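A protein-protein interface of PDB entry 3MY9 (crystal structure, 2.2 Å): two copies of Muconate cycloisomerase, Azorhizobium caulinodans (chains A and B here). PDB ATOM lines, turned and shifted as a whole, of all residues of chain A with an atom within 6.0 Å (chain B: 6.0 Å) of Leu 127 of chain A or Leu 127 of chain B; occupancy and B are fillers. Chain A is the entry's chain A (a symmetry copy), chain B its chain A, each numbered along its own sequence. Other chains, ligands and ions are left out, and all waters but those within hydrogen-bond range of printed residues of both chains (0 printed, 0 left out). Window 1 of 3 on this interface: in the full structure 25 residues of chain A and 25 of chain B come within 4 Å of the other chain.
Leu 116 of chain A touches none of the printed residues of chain B.
Printed residues of chain B within 4 Å of Thr 120 of chain A: Thr 120 and Leu 122.
Of chain B, only Leu 127 comes within 4 Å of Leu 127 of chain A.
Of the printed residues of chain B, Gly 129 of chain A touches Met 280.
Of the printed residues of chain B, Met 280 of chain A touches Gly 129 (3.8 Å).
Leu 127 of chain B touches one residue of chain A.
Of the printed residues of chain A, Gly 129 of chain B touches Met 280 (3.8 Å).
The nearest residue of chain B that does not touch Leu 127 of chain A is Leu 122 of chain B (4.1 Å).
The nearest residue of chain A that does not touch Leu 127 of chain B is Leu 122 of chain A (4.1 Å).
The nearest printed residue of chain B that does not touch Thr 120 of chain A is Leu 116 of chain B (6.8 Å).
Thr 120 of chain B touches its own counterpart, Thr 120 of chain A.
Thr 120 of chain A touches Leu 122 of chain B, and with the chains exchanged Leu 122 of chain A touches Thr 120 of chain B.
Leu 127 of chain B touches its own counterpart, Leu 127 of chain A.
Gly 129 of chain A touches Met 280 of chain B, and with the chains exchanged Met 280 of chain A touches Gly 129 of chain B.
Positions printed for both chains: 113, 114, 116, 117, 120, 122, 123, 124, 125, 126, 127, 128, 129, 130, 280 and 283.
Of the 6 pairs that touch across the chains among the printed residues, 6 have their exchanged pair printed and touching as well.
Printed residues of chain B that touch a printed residue of chain A: Thr 120, Leu 122, Leu 127, Gly 129 and Met 280.
O of Leu 116 of chain A lies within hydrogen-bond range of OG1 of Thr 120 of chain A, 2.6 Å away.
The side-chain hydroxyl (OG1) of Thr 120 of chain B lies within hydrogen-bond range of the backbone carbonyl oxygen (O) of Gly 117 of chain B (3.3 Å).
The backbone carbonyl oxygen (O) of Gly 117 of chain A is in hydrogen-bond range of the backbone NH (N) of Leu 122 of chain A, at 2.9 Å.
The backbone carbonyl oxygen (O) of Gly 117 of chain B sits at hydrogen-bond distance from the backbone NH (N) of Leu 122 of chain B (2.9 Å).
OG1 of Thr 120 of chain A is in hydrogen-bond range of O of Gly 117 of chain A, at 3.3 Å.
The backbone carbonyl oxygen (O) of Leu 116 of chain B lies within hydrogen-bond range of the side-chain hydroxyl (OG1) of Thr 120 of chain B (2.6 Å).
O of Thr 120 of chain A touches CG2 of Thr 120 of chain B, at 3.4 Å.
Leu 122 of chain B touches Thr 120 of chain A (CG to CG2, 3.8 Å).
CG2 of Thr 120 of chain B touches CG of Leu 122 of chain A (3.8 Å).
Leu 127 of chain B touches Leu 127 of chain A (O to O, 3.9 Å).
Met 280 of chain B touches Gly 129 of chain A.
Gly 129 of chain B touches Met 280 of chain A.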
ATOM      1  N   LEU A 113     -18.441  -5.816  -5.399  1.00  0.00           N
ATOM      2  CA  LEU A 113     -19.092  -6.956  -6.032  1.00  0.00           C
ATOM      3  C   LEU A 113     -19.972  -6.524  -7.216  1.00  0.00           C
ATOM      4  O   LEU A 113     -20.054  -7.245  -8.212  1.00  0.00           O
ATOM      5  CB  LEU A 113     -19.897  -7.772  -5.004  1.00  0.00           C
ATOM      6  CG  LEU A 113     -19.085  -8.384  -3.860  1.00  0.00           C
ATOM      7  CD1 LEU A 113     -19.940  -9.175  -2.833  1.00  0.00           C
ATOM      8  CD2 LEU A 113     -17.966  -9.278  -4.419  1.00  0.00           C
ATOM      9  N   ASP A 114     -20.600  -5.344  -7.115  1.00  0.00           N
ATOM     10  CA  ASP A 114     -21.357  -4.739  -8.222  1.00  0.00           C
ATOM     11  C   ASP A 114     -20.424  -4.516  -9.433  1.00  0.00           C
ATOM     12  O   ASP A 114     -20.711  -4.957 -10.544  1.00  0.00           O
ATOM     13  CB  ASP A 114     -21.971  -3.415  -7.749  1.00  0.00           C
ATOM     14  CG  ASP A 114     -23.097  -2.893  -8.657  1.00  0.00           C
ATOM     15  OD1 ASP A 114     -23.717  -3.663  -9.432  1.00  0.00           O
ATOM     16  OD2 ASP A 114     -23.391  -1.685  -8.544  1.00  0.00           O
ATOM     17  N   LEU A 116     -17.307  -5.840  -9.947  1.00  0.00           N
ATOM     18  CA  LEU A 116     -16.772  -7.142 -10.381  1.00  0.00           C
ATOM     19  C   LEU A 116     -17.781  -7.901 -11.237  1.00  0.00           C
ATOM     20  O   LEU A 116     -17.435  -8.472 -12.275  1.00  0.00           O
ATOM     21  CB  LEU A 116     -16.394  -7.986  -9.162  1.00  0.00           C
ATOM     22  CG  LEU A 116     -15.719  -9.327  -9.416  1.00  0.00           C
ATOM     23  CD1 LEU A 116     -14.456  -9.170 -10.270  1.00  0.00           C
ATOM     24  CD2 LEU A 116     -15.381  -9.998  -8.053  1.00  0.00           C
ATOM     25  N   GLY A 117     -19.036  -7.880 -10.806  1.00  0.00           N
ATOM     26  CA  GLY A 117     -20.102  -8.501 -11.565  1.00  0.00           C
ATOM     27  C   GLY A 117     -20.288  -7.898 -12.955  1.00  0.00           C
ATOM     28  O   GLY A 117     -20.387  -8.630 -13.949  1.00  0.00           O
ATOM     29  N   THR A 120     -17.560  -8.728 -15.432  1.00  0.00           N
ATOM     30  CA  THR A 120     -17.437 -10.111 -15.843  1.00  0.00           C
ATOM     31  C   THR A 120     -18.722 -10.727 -16.387  1.00  0.00           C
ATOM     32  O   THR A 120     -18.718 -11.899 -16.768  1.00  0.00           O
ATOM     33  CB  THR A 120     -16.959 -10.952 -14.650  1.00  0.00           C
ATOM     34  OG1 THR A 120     -17.806 -10.712 -13.514  1.00  0.00           O
ATOM     35  CG2 THR A 120     -15.537 -10.582 -14.303  1.00  0.00           C
ATOM     36  N   LEU A 122     -21.464 -11.220 -14.544  1.00  0.00           N
ATOM     37  CA  LEU A 122     -22.015 -12.055 -13.490  1.00  0.00           C
ATOM     38  C   LEU A 122     -22.804 -11.211 -12.507  1.00  0.00           C
ATOM     39  O   LEU A 122     -22.432 -10.074 -12.214  1.00  0.00           O
ATOM     40  CB  LEU A 122     -20.883 -12.763 -12.720  1.00  0.00           C
ATOM     41  CG  LEU A 122     -20.131 -13.878 -13.456  1.00  0.00           C
ATOM     42  CD1 LEU A 122     -18.974 -14.417 -12.571  1.00  0.00           C
ATOM     43  CD2 LEU A 122     -21.081 -15.006 -13.884  1.00  0.00           C
ATOM     44  N   SER A 123     -23.877 -11.779 -11.976  1.00  0.00           N
ATOM     45  CA  SER A 123     -24.553 -11.183 -10.837  1.00  0.00           C
ATOM     46  C   SER A 123     -23.765 -11.428  -9.540  1.00  0.00           C
ATOM     47  O   SER A 123     -22.858 -12.278  -9.472  1.00  0.00           O
ATOM     48  CB  SER A 123     -25.934 -11.786 -10.678  1.00  0.00           C
ATOM     49  OG  SER A 123     -25.850 -13.153 -10.318  1.00  0.00           O
ATOM     50  N   VAL A 124     -24.154 -10.708  -8.495  1.00  0.00           N
ATOM     51  CA  VAL A 124     -23.603 -10.923  -7.184  1.00  0.00           C
ATOM     52  C   VAL A 124     -23.916 -12.343  -6.677  1.00  0.00           C
ATOM     53  O   VAL A 124     -23.034 -13.011  -6.140  1.00  0.00           O
ATOM     54  CB  VAL A 124     -24.050  -9.802  -6.222  1.00  0.00           C
ATOM     55  CG1 VAL A 124     -23.695 -10.147  -4.811  1.00  0.00           C
ATOM     56  CG2 VAL A 124     -23.380  -8.481  -6.652  1.00  0.00           C
ATOM     57  N   ALA A 125     -25.145 -12.822  -6.859  1.00  0.00           N
ATOM     58  CA  ALA A 125     -25.458 -14.232  -6.549  1.00  0.00           C
ATOM     59  C   ALA A 125     -24.449 -15.207  -7.203  1.00  0.00           C
ATOM     60  O   ALA A 125     -23.975 -16.133  -6.560  1.00  0.00           O
ATOM     61  CB  ALA A 125     -26.875 -14.574  -6.989  1.00  0.00           C
ATOM     62  N   ASP A 126     -24.165 -14.992  -8.487  1.00  0.00           N
ATOM     63  CA  ASP A 126     -23.207 -15.799  -9.263  1.00  0.00           C
ATOM     64  C   ASP A 126     -21.827 -15.866  -8.607  1.00  0.00           C
ATOM     65  O   ASP A 126     -21.180 -16.895  -8.653  1.00  0.00           O
ATOM     66  CB  ASP A 126     -22.988 -15.202 -10.668  1.00  0.00           C
ATOM     67  CG  ASP A 126     -24.236 -15.177 -11.526  1.00  0.00           C
ATOM     68  OD1 ASP A 126     -25.130 -16.013 -11.299  1.00  0.00           O
ATOM     69  OD2 ASP A 126     -24.295 -14.335 -12.468  1.00  0.00           O
ATOM     70  N   LEU A 127     -21.384 -14.734  -8.068  1.00  0.00           N
ATOM     71  CA  LEU A 127     -20.110 -14.595  -7.380  1.00  0.00           C
ATOM     72  C   LEU A 127     -20.110 -15.146  -5.948  1.00  0.00           C
ATOM     73  O   LEU A 127     -19.057 -15.134  -5.265  1.00  0.00           O
ATOM     74  CB  LEU A 127     -19.731 -13.119  -7.332  1.00  0.00           C
ATOM     75  CG  LEU A 127     -19.495 -12.479  -8.705  1.00  0.00           C
ATOM     76  CD1 LEU A 127     -19.407 -10.969  -8.572  1.00  0.00           C
ATOM     77  CD2 LEU A 127     -18.223 -13.064  -9.313  1.00  0.00           C
ATOM     78  N   LEU A 128     -21.283 -15.578  -5.483  1.00  0.00           N
ATOM     79  CA  LEU A 128     -21.463 -16.106  -4.139  1.00  0.00           C
ATOM     80  C   LEU A 128     -21.858 -17.587  -4.179  1.00  0.00           C
ATOM     81  O   LEU A 128     -22.447 -18.116  -3.229  1.00  0.00           O
ATOM     82  CB  LEU A 128     -22.542 -15.280  -3.405  1.00  0.00           C
ATOM     83  CG  LEU A 128     -22.112 -13.835  -3.110  1.00  0.00           C
ATOM     84  CD1 LEU A 128     -23.201 -13.083  -2.362  1.00  0.00           C
ATOM     85  CD2 LEU A 128     -20.779 -13.778  -2.348  1.00  0.00           C
ATOM     86  N   GLY A 129     -21.560 -18.235  -5.311  1.00  0.00           N
ATOM     87  CA  GLY A 129     -21.758 -19.669  -5.471  1.00  0.00           C
ATOM     88  C   GLY A 129     -22.877 -20.012  -6.424  1.00  0.00           C
ATOM     89  O   GLY A 129     -23.113 -21.187  -6.693  1.00  0.00           O
ATOM     90  N   GLY A 130     -23.570 -18.988  -6.913  1.00  0.00           N
ATOM     91  CA  GLY A 130     -24.670 -19.153  -7.832  1.00  0.00           C
ATOM     92  C   GLY A 130     -26.017 -19.133  -7.133  1.00  0.00           C
ATOM     93  O   GLY A 130     -26.120 -19.480  -5.963  1.00  0.00           O
ATOM     94  N   MET A 280     -20.434 -11.856   2.402  1.00  0.00           N
ATOM     95  CA  MET A 280     -19.582 -13.035   2.647  1.00  0.00           C
ATOM     96  C   MET A 280     -19.696 -13.497   4.116  1.00  0.00           C
ATOM     97  O   MET A 280     -19.763 -14.686   4.377  1.00  0.00           O
ATOM     98  CB  MET A 280     -18.117 -12.789   2.242  1.00  0.00           C
ATOM     99  CG  MET A 280     -17.902 -12.687   0.685  1.00  0.00           C
ATOM    100  SD  MET A 280     -16.175 -12.561   0.049  1.00  0.00           S
ATOM    101  CE  MET A 280     -16.717 -12.122  -1.615  1.00  0.00           C
ATOM    102  N   GLN A 283     -22.840 -15.504   4.576  1.00  0.00           N
ATOM    103  CA  GLN A 283     -22.714 -16.886   4.084  1.00  0.00           C
ATOM    104  C   GLN A 283     -21.849 -17.743   5.020  1.00  0.00           C
ATOM    105  O   GLN A 283     -22.075 -18.937   5.142  1.00  0.00           O
ATOM    106  CB  GLN A 283     -22.152 -16.909   2.676  1.00  0.00           C
ATOM    107  CG  GLN A 283     -23.126 -16.440   1.600  1.00  0.00           C
ATOM    108  CD  GLN A 283     -22.723 -16.926   0.203  1.00  0.00           C
ATOM    109  OE1 GLN A 283     -21.545 -16.912  -0.140  1.00  0.00           O
ATOM    110  NE2 GLN A 283     -23.707 -17.360  -0.594  1.00  0.00           N
ATOM    111  N   LEU B 113     -16.321 -24.748 -12.320  1.00  0.00           N
ATOM    112  CA  LEU B 113     -15.645 -23.521 -11.918  1.00  0.00           C
ATOM    113  C   LEU B 113     -14.534 -23.133 -12.906  1.00  0.00           C
ATOM    114  O   LEU B 113     -14.319 -21.943 -13.149  1.00  0.00           O
ATOM    115  CB  LEU B 113     -15.103 -23.635 -10.482  1.00  0.00           C
ATOM    116  CG  LEU B 113     -16.154 -23.866  -9.393  1.00  0.00           C
ATOM    117  CD1 LEU B 113     -15.561 -24.002  -7.963  1.00  0.00           C
ATOM    118  CD2 LEU B 113     -17.210 -22.749  -9.424  1.00  0.00           C
ATOM    119  N   ASP B 114     -13.854 -24.131 -13.488  1.00  0.00           N
ATOM    120  CA  ASP B 114     -12.865 -23.915 -14.555  1.00  0.00           C
ATOM    121  C   ASP B 114     -13.540 -23.225 -15.762  1.00  0.00           C
ATOM    122  O   ASP B 114     -13.084 -22.186 -16.234  1.00  0.00           O
ATOM    123  CB  ASP B 114     -12.259 -25.264 -14.961  1.00  0.00           C
ATOM    124  CG  ASP B 114     -10.950 -25.141 -15.760  1.00  0.00           C
ATOM    125  OD1 ASP B 114     -10.252 -24.099 -15.709  1.00  0.00           O
ATOM    126  OD2 ASP B 114     -10.598 -26.145 -16.414  1.00  0.00           O
ATOM    127  N   LEU B 116     -16.593 -21.675 -15.849  1.00  0.00           N
ATOM    128  CA  LEU B 116     -17.128 -20.372 -15.414  1.00  0.00           C
ATOM    129  C   LEU B 116     -16.033 -19.311 -15.358  1.00  0.00           C
ATOM    130  O   LEU B 116     -16.220 -18.178 -15.810  1.00  0.00           O
ATOM    131  CB  LEU B 116     -17.782 -20.508 -14.038  1.00  0.00           C
ATOM    132  CG  LEU B 116     -18.491 -19.285 -13.472  1.00  0.00           C
ATOM    133  CD1 LEU B 116     -19.560 -18.756 -14.434  1.00  0.00           C
ATOM    134  CD2 LEU B 116     -19.122 -19.648 -12.096  1.00  0.00           C
ATOM    135  N   GLY B 117     -14.881 -19.697 -14.824  1.00  0.00           N
ATOM    136  CA  GLY B 117     -13.739 -18.808 -14.777  1.00  0.00           C
ATOM    137  C   GLY B 117     -13.258 -18.364 -16.156  1.00  0.00           C
ATOM    138  O   GLY B 117     -13.028 -17.170 -16.387  1.00  0.00           O
ATOM    139  N   THR B 120     -15.531 -15.928 -17.934  1.00  0.00           N
ATOM    140  CA  THR B 120     -15.673 -14.609 -17.353  1.00  0.00           C
ATOM    141  C   THR B 120     -14.356 -13.879 -17.111  1.00  0.00           C
ATOM    142  O   THR B 120     -14.370 -12.748 -16.624  1.00  0.00           O
ATOM    143  CB  THR B 120     -16.421 -14.723 -16.016  1.00  0.00           C
ATOM    144  OG1 THR B 120     -15.784 -15.706 -15.184  1.00  0.00           O
ATOM    145  CG2 THR B 120     -17.853 -15.130 -16.267  1.00  0.00           C
ATOM    146  N   LEU B 122     -12.043 -14.906 -14.930  1.00  0.00           N
ATOM    147  CA  LEU B 122     -11.757 -15.005 -13.509  1.00  0.00           C
ATOM    148  C   LEU B 122     -11.106 -16.339 -13.194  1.00  0.00           C
ATOM    149  O   LEU B 122     -11.445 -17.361 -13.792  1.00  0.00           O
ATOM    150  CB  LEU B 122     -13.057 -14.897 -12.691  1.00  0.00           C
ATOM    151  CG  LEU B 122     -13.736 -13.523 -12.639  1.00  0.00           C
ATOM    152  CD1 LEU B 122     -15.072 -13.616 -11.851  1.00  0.00           C
ATOM    153  CD2 LEU B 122     -12.805 -12.460 -12.039  1.00  0.00           C
ATOM    154  N   SER B 123     -10.192 -16.334 -12.235  1.00  0.00           N
ATOM    155  CA  SER B 123      -9.698 -17.575 -11.665  1.00  0.00           C
ATOM    156  C   SER B 123     -10.728 -18.184 -10.699  1.00  0.00           C
ATOM    157  O   SER B 123     -11.689 -17.526 -10.261  1.00  0.00           O
ATOM    158  CB  SER B 123      -8.416 -17.322 -10.898  1.00  0.00           C
ATOM    159  OG  SER B 123      -8.660 -16.522  -9.755  1.00  0.00           O
ATOM    160  N   VAL B 124     -10.490 -19.438 -10.332  1.00  0.00           N
ATOM    161  CA  VAL B 124     -11.287 -20.095  -9.332  1.00  0.00           C
ATOM    162  C   VAL B 124     -11.173 -19.379  -7.974  1.00  0.00           C
ATOM    163  O   VAL B 124     -12.184 -19.166  -7.306  1.00  0.00           O
ATOM    164  CB  VAL B 124     -10.949 -21.599  -9.278  1.00  0.00           C
ATOM    165  CG1 VAL B 124     -11.582 -22.238  -8.084  1.00  0.00           C
ATOM    166  CG2 VAL B 124     -11.434 -22.266 -10.581  1.00  0.00           C
ATOM    167  N   ALA B 125      -9.968 -18.986  -7.566  1.00  0.00           N
ATOM    168  CA  ALA B 125      -9.818 -18.148  -6.358  1.00  0.00           C
ATOM    169  C   ALA B 125     -10.754 -16.916  -6.386  1.00  0.00           C
ATOM    170  O   ALA B 125     -11.402 -16.606  -5.396  1.00  0.00           O
ATOM    171  CB  ALA B 125      -8.371 -17.702  -6.195  1.00  0.00           C
ATOM    172  N   ASP B 126     -10.780 -16.217  -7.521  1.00  0.00           N
ATOM    173  CA  ASP B 126     -11.632 -15.035  -7.739  1.00  0.00           C
ATOM    174  C   ASP B 126     -13.110 -15.317  -7.470  1.00  0.00           C
ATOM    175  O   ASP B 126     -13.808 -14.468  -6.950  1.00  0.00           O
ATOM    176  CB  ASP B 126     -11.545 -14.550  -9.200  1.00  0.00           C
ATOM    177  CG  ASP B 126     -10.160 -14.095  -9.614  1.00  0.00           C
ATOM    178  OD1 ASP B 126      -9.385 -13.677  -8.736  1.00  0.00           O
ATOM    179  OD2 ASP B 126      -9.870 -14.116 -10.846  1.00  0.00           O
ATOM    180  N   LEU B 127     -13.566 -16.492  -7.897  1.00  0.00           N
ATOM    181  CA  LEU B 127     -14.931 -16.958  -7.720  1.00  0.00           C
ATOM    182  C   LEU B 127     -15.235 -17.480  -6.309  1.00  0.00           C
ATOM    183  O   LEU B 127     -16.393 -17.862  -6.011  1.00  0.00           O
ATOM    184  CB  LEU B 127     -15.209 -18.074  -8.720  1.00  0.00           C
ATOM    185  CG  LEU B 127     -15.142 -17.641 -10.189  1.00  0.00           C
ATOM    186  CD1 LEU B 127     -15.147 -18.859 -11.095  1.00  0.00           C
ATOM    187  CD2 LEU B 127     -16.317 -16.714 -10.488  1.00  0.00           C
ATOM    188  N   LEU B 128     -14.201 -17.541  -5.468  1.00  0.00           N
ATOM    189  CA  LEU B 128     -14.311 -18.035  -4.104  1.00  0.00           C
ATOM    190  C   LEU B 128     -14.020 -16.921  -3.091  1.00  0.00           C
ATOM    191  O   LEU B 128     -13.655 -17.186  -1.939  1.00  0.00           O
ATOM    192  CB  LEU B 128     -13.331 -19.213  -3.906  1.00  0.00           C
ATOM    193  CG  LEU B 128     -13.706 -20.464  -4.716  1.00  0.00           C
ATOM    194  CD1 LEU B 128     -12.725 -21.596  -4.457  1.00  0.00           C
ATOM    195  CD2 LEU B 128     -15.150 -20.912  -4.440  1.00  0.00           C
ATOM    196  N   GLY B 129     -14.147 -15.672  -3.552  1.00  0.00           N
ATOM    197  CA  GLY B 129     -14.024 -14.502  -2.694  1.00  0.00           C
ATOM    198  C   GLY B 129     -12.775 -13.698  -2.962  1.00  0.00           C
ATOM    199  O   GLY B 129     -12.576 -12.654  -2.347  1.00  0.00           O
ATOM    200  N   GLY B 130     -11.933 -14.197  -3.862  1.00  0.00           N
ATOM    201  CA  GLY B 130     -10.697 -13.549  -4.224  1.00  0.00           C
ATOM    202  C   GLY B 130      -9.504 -14.115  -3.476  1.00  0.00           C
ATOM    203  O   GLY B 130      -9.644 -14.627  -2.372  1.00  0.00           O
ATOM    204  N   MET B 280     -16.232 -25.444  -2.279  1.00  0.00           N
ATOM    205  CA  MET B 280     -17.195 -24.657  -1.486  1.00  0.00           C
ATOM    206  C   MET B 280     -17.388 -25.278  -0.085  1.00  0.00           C
ATOM    207  O   MET B 280     -17.454 -24.558   0.897  1.00  0.00           O
ATOM    208  CB  MET B 280     -18.540 -24.474  -2.215  1.00  0.00           C
ATOM    209  CG  MET B 280     -18.455 -23.518  -3.463  1.00  0.00           C
ATOM    210  SD  MET B 280     -20.022 -23.076  -4.331  1.00  0.00           S
ATOM    211  CE  MET B 280     -19.152 -22.355  -5.739  1.00  0.00           C
ATOM    212  N   GLN B 283     -14.531 -24.287   2.147  1.00  0.00           N
ATOM    213  CA  GLN B 283     -14.660 -22.916   2.666  1.00  0.00           C
ATOM    214  C   GLN B 283     -15.741 -22.823   3.755  1.00  0.00           C
ATOM    215  O   GLN B 283     -15.626 -22.020   4.666  1.00  0.00           O
ATOM    216  CB  GLN B 283     -14.953 -21.938   1.546  1.00  0.00           C
ATOM    217  CG  GLN B 283     -13.766 -21.656   0.630  1.00  0.00           C
ATOM    218  CD  GLN B 283     -13.936 -20.347  -0.150  1.00  0.00           C
ATOM    219  OE1 GLN B 283     -15.027 -20.051  -0.629  1.00  0.00           O
ATOM    220  NE2 GLN B 283     -12.854 -19.567  -0.269  1.00  0.00           N
